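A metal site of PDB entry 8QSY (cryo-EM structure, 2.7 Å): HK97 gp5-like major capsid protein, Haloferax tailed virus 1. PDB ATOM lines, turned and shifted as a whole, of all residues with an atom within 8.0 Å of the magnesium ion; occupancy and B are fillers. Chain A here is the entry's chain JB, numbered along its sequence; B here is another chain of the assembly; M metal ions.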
ATOM      1  N   ASP A 259      10.989   9.939  19.588  1.00  0.00           N
ATOM      2  CA  ASP A 259      10.757  10.786  18.427  1.00  0.00           C
ATOM      3  C   ASP A 259      12.030  11.467  17.912  1.00  0.00           C
ATOM      4  O   ASP A 259      11.983  12.171  16.906  1.00  0.00           O
ATOM      5  CB  ASP A 259       9.662  11.819  18.716  1.00  0.00           C
ATOM      6  CG  ASP A 259       9.998  12.842  19.798  1.00  0.00           C
ATOM      7  OD1 ASP A 259      11.145  12.847  20.304  1.00  0.00           O
ATOM      8  OD2 ASP A 259       9.094  13.647  20.116  1.00  0.00           O
ATOM      9  N   ILE A 297      15.475  12.619   4.812  1.00  0.00           N
ATOM     10  CA  ILE A 297      15.169  11.293   5.340  1.00  0.00           C
ATOM     11  C   ILE A 297      15.945  10.968   6.627  1.00  0.00           C
ATOM     12  O   ILE A 297      15.465  10.196   7.454  1.00  0.00           O
ATOM     13  CB  ILE A 297      15.351  10.192   4.260  1.00  0.00           C
ATOM     14  CG1 ILE A 297      14.895   8.830   4.776  1.00  0.00           C
ATOM     15  CG2 ILE A 297      16.777  10.152   3.734  1.00  0.00           C
ATOM     16  CD1 ILE A 297      14.414   7.854   3.712  1.00  0.00           C
ATOM     17  N   GLY A 299      16.435  12.879   9.154  1.00  0.00           N
ATOM     18  CA  GLY A 299      15.572  13.394  10.213  1.00  0.00           C
ATOM     19  C   GLY A 299      14.122  12.895  10.134  1.00  0.00           C
ATOM     20  O   GLY A 299      13.243  13.513  10.726  1.00  0.00           O
ATOM     21  N   ASP A 300      13.877  11.791   9.416  1.00  0.00           N
ATOM     22  CA  ASP A 300      12.542  11.230   9.231  1.00  0.00           C
ATOM     23  C   ASP A 300      12.692   9.719   8.993  1.00  0.00           C
ATOM     24  O   ASP A 300      12.429   9.234   7.903  1.00  0.00           O
ATOM     25  CB  ASP A 300      11.809  11.927   8.088  1.00  0.00           C
ATOM     26  CG  ASP A 300      10.338  11.560   7.940  1.00  0.00           C
ATOM     27  OD1 ASP A 300       9.719  11.157   8.955  1.00  0.00           O
ATOM     28  OD2 ASP A 300       9.803  11.703   6.812  1.00  0.00           O
ATOM     29  N   ILE A 301      13.176   8.995  10.011  1.00  0.00           N
ATOM     30  CA  ILE A 301      13.535   7.585   9.907  1.00  0.00           C
ATOM     31  C   ILE A 301      13.042   6.822  11.141  1.00  0.00           C
ATOM     32  O   ILE A 301      13.088   7.341  12.243  1.00  0.00           O
ATOM     33  CB  ILE A 301      15.056   7.417   9.712  1.00  0.00           C
ATOM     34  CG1 ILE A 301      15.441   5.962   9.415  1.00  0.00           C
ATOM     35  CG2 ILE A 301      15.848   7.984  10.895  1.00  0.00           C
ATOM     36  CD1 ILE A 301      16.866   5.775   8.941  1.00  0.00           C
ATOM     37  N   ALA A 302      12.559   5.581  10.950  1.00  0.00           N
ATOM     38  CA  ALA A 302      12.150   4.710  12.050  1.00  0.00           C
ATOM     39  C   ALA A 302      11.114   5.367  12.987  1.00  0.00           C
ATOM     40  O   ALA A 302      11.054   5.016  14.169  1.00  0.00           O
ATOM     41  CB  ALA A 302      13.382   4.197  12.797  1.00  0.00           C
ATOM     42  N   GLY A 303      10.292   6.293  12.476  1.00  0.00           N
ATOM     43  CA  GLY A 303       9.299   6.988  13.284  1.00  0.00           C
ATOM     44  C   GLY A 303       9.844   8.177  14.080  1.00  0.00           C
ATOM     45  O   GLY A 303       9.062   8.908  14.696  1.00  0.00           O
ATOM     46  N   LEU A 304      11.169   8.400  14.025  1.00  0.00           N
ATOM     47  CA  LEU A 304      11.845   9.541  14.625  1.00  0.00           C
ATOM     48  C   LEU A 304      11.788  10.700  13.643  1.00  0.00           C
ATOM     49  O   LEU A 304      12.267  10.587  12.519  1.00  0.00           O
ATOM     50  CB  LEU A 304      13.299   9.145  14.941  1.00  0.00           C
ATOM     51  CG  LEU A 304      13.460   7.825  15.690  1.00  0.00           C
ATOM     52  CD1 LEU A 304      14.923   7.435  15.784  1.00  0.00           C
ATOM     53  CD2 LEU A 304      12.856   7.901  17.080  1.00  0.00           C
ATOM     54  N   ASP A 305      11.240  11.827  14.091  1.00  0.00           N
ATOM     55  CA  ASP A 305      11.033  13.011  13.257  1.00  0.00           C
ATOM     56  C   ASP A 305      12.091  14.090  13.497  1.00  0.00           C
ATOM     57  O   ASP A 305      11.915  15.233  13.060  1.00  0.00           O
ATOM     58  CB  ASP A 305       9.586  13.510  13.391  1.00  0.00           C
ATOM     59  CG  ASP A 305       8.500  12.604  12.805  1.00  0.00           C
ATOM     60  OD1 ASP A 305       8.712  12.058  11.695  1.00  0.00           O
ATOM     61  OD2 ASP A 305       7.407  12.525  13.425  1.00  0.00           O
ATOM     62  N   MET A 306      13.200  13.759  14.191  1.00  0.00           N
ATOM     63  CA  MET A 306      14.310  14.683  14.374  1.00  0.00           C
ATOM     64  C   MET A 306      15.644  13.949  14.572  1.00  0.00           C
ATOM     65  O   MET A 306      15.729  13.022  15.372  1.00  0.00           O
ATOM     66  CB  MET A 306      14.062  15.601  15.570  1.00  0.00           C
ATOM     67  CG  MET A 306      15.194  16.573  15.801  1.00  0.00           C
ATOM     68  SD  MET A 306      14.938  17.786  17.109  1.00  0.00           S
ATOM     69  CE  MET A 306      16.557  18.547  17.082  1.00  0.00           C
ATOM     70  N   GLU B 287       7.429   4.742   3.302  1.00  0.00           N
ATOM     71  CA  GLU B 287       6.696   5.096   4.498  1.00  0.00           C
ATOM     72  C   GLU B 287       7.080   4.241   5.711  1.00  0.00           C
ATOM     73  O   GLU B 287       7.235   4.784   6.796  1.00  0.00           O
ATOM     74  CB  GLU B 287       5.188   5.069   4.246  1.00  0.00           C
ATOM     75  CG  GLU B 287       4.671   6.309   3.542  1.00  0.00           C
ATOM     76  CD  GLU B 287       4.584   7.558   4.398  1.00  0.00           C
ATOM     77  OE1 GLU B 287       4.568   7.430   5.649  1.00  0.00           O
ATOM     78  OE2 GLU B 287       4.550   8.677   3.834  1.00  0.00           O
ATOM     79  N   LEU B 289      10.044   2.720   6.268  1.00  0.00           N
ATOM     80  CA  LEU B 289      11.387   3.159   6.613  1.00  0.00           C
ATOM     81  C   LEU B 289      11.388   4.510   7.339  1.00  0.00           C
ATOM     82  O   LEU B 289      12.147   4.699   8.294  1.00  0.00           O
ATOM     83  CB  LEU B 289      12.204   3.216   5.312  1.00  0.00           C
ATOM     84  CG  LEU B 289      13.602   3.811   5.380  1.00  0.00           C
ATOM     85  CD1 LEU B 289      14.482   3.044   6.362  1.00  0.00           C
ATOM     86  CD2 LEU B 289      14.239   3.793   3.998  1.00  0.00           C
ATOM     87  N   ARG B 290      10.507   5.425   6.944  1.00  0.00           N
ATOM     88  CA  ARG B 290      10.438   6.762   7.535  1.00  0.00           C
ATOM     89  C   ARG B 290       9.614   6.812   8.816  1.00  0.00           C
ATOM     90  O   ARG B 290      10.072   7.326   9.829  1.00  0.00           O
ATOM     91  CB  ARG B 290       9.913   7.769   6.512  1.00  0.00           C
ATOM     92  CG  ARG B 290      10.909   7.981   5.373  1.00  0.00           C
ATOM     93  CD  ARG B 290      10.596   9.239   4.576  1.00  0.00           C
ATOM     94  NE  ARG B 290       9.388   9.075   3.796  1.00  0.00           N
ATOM     95  CZ  ARG B 290       8.196   9.608   4.028  1.00  0.00           C
ATOM     96  NH1 ARG B 290       7.206   9.306   3.208  1.00  0.00           N
ATOM     97  NH2 ARG B 290       7.958  10.419   5.048  1.00  0.00           N
ATOM     98  N   ASN B 291       8.383   6.288   8.773  1.00  0.00           N
ATOM     99  CA  ASN B 291       7.364   6.533   9.782  1.00  0.00           C
ATOM    100  C   ASN B 291       6.990   5.295  10.608  1.00  0.00           C
ATOM    101  O   ASN B 291       6.161   5.416  11.514  1.00  0.00           O
ATOM    102  CB  ASN B 291       6.159   7.218   9.138  1.00  0.00           C
ATOM    103  CG  ASN B 291       6.517   8.605   8.655  1.00  0.00           C
ATOM    104  OD1 ASN B 291       7.134   9.381   9.371  1.00  0.00           O
ATOM    105  ND2 ASN B 291       6.113   8.936   7.445  1.00  0.00           N
ATOM    106  N   ARG B 292       7.583   4.121  10.332  1.00  0.00           N
ATOM    107  CA  ARG B 292       7.418   2.920  11.162  1.00  0.00           C
ATOM    108  C   ARG B 292       5.937   2.552  11.297  1.00  0.00           C
ATOM    109  O   ARG B 292       5.267   2.393  10.282  1.00  0.00           O
ATOM    110  CB  ARG B 292       8.201   3.063  12.474  1.00  0.00           C
ATOM    111  CG  ARG B 292       8.628   1.747  13.097  1.00  0.00           C
ATOM    112  CD  ARG B 292       9.376   1.988  14.380  1.00  0.00           C
ATOM    113  NE  ARG B 292       9.961   0.761  14.880  1.00  0.00           N
ATOM    114  CZ  ARG B 292       9.502   0.031  15.890  1.00  0.00           C
ATOM    115  NH1 ARG B 292      10.150  -1.076  16.218  1.00  0.00           N
ATOM    116  NH2 ARG B 292       8.425   0.387  16.573  1.00  0.00           N
ATOM    117  N   ASP B 294       3.344   4.267  11.904  1.00  0.00           N
ATOM    118  CA  ASP B 294       2.441   5.290  11.403  1.00  0.00           C
ATOM    119  C   ASP B 294       2.298   5.250   9.879  1.00  0.00           C
ATOM    120  O   ASP B 294       1.494   5.992   9.310  1.00  0.00           O
ATOM    121  CB  ASP B 294       2.928   6.636  11.924  1.00  0.00           C
ATOM    122  CG  ASP B 294       1.958   7.792  11.734  1.00  0.00           C
ATOM    123  OD1 ASP B 294       0.751   7.587  11.975  1.00  0.00           O
ATOM    124  OD2 ASP B 294       2.417   8.889  11.346  1.00  0.00           O
HETATM  125 MG    MG M   1       8.172  10.910  10.143  1.00  0.00          MG
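The side-chain carboxylate of Asp 300 is in salt-bridge range of the guanidinium group of Arg 290 of chain B, 2.9 Å away.
The guanidinium group of Arg 290 of chain B sits close to the side-chain amide nitrogen of Asn 291 of chain B (3.4 Å).
The side-chain amide nitrogen of Asn 291 of chain B sits at hydrogen-bond distance from the side-chain carboxylate of Glu 287 of chain B, 2.8 Å away.
N of Asp 305 lies within hydrogen-bond range of O of Asp 259 (2.9 Å).
Three residues have an atom within 4 Å of the magnesium ion: Asp 300, Asp 305 and Asn 291 of chain B.
The nearest printed residue that does not touch the magnesium ion is Arg 290 of chain B (4.1 Å).
The magnesium ion is bound by OD1 of Asp 300 (2.0 Å), OD1 of Asn 291 of chain B (2.0 Å) and OD1 of Asp 305 (2.0 Å).
The magnesium ion has three donor atoms within binding distance.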
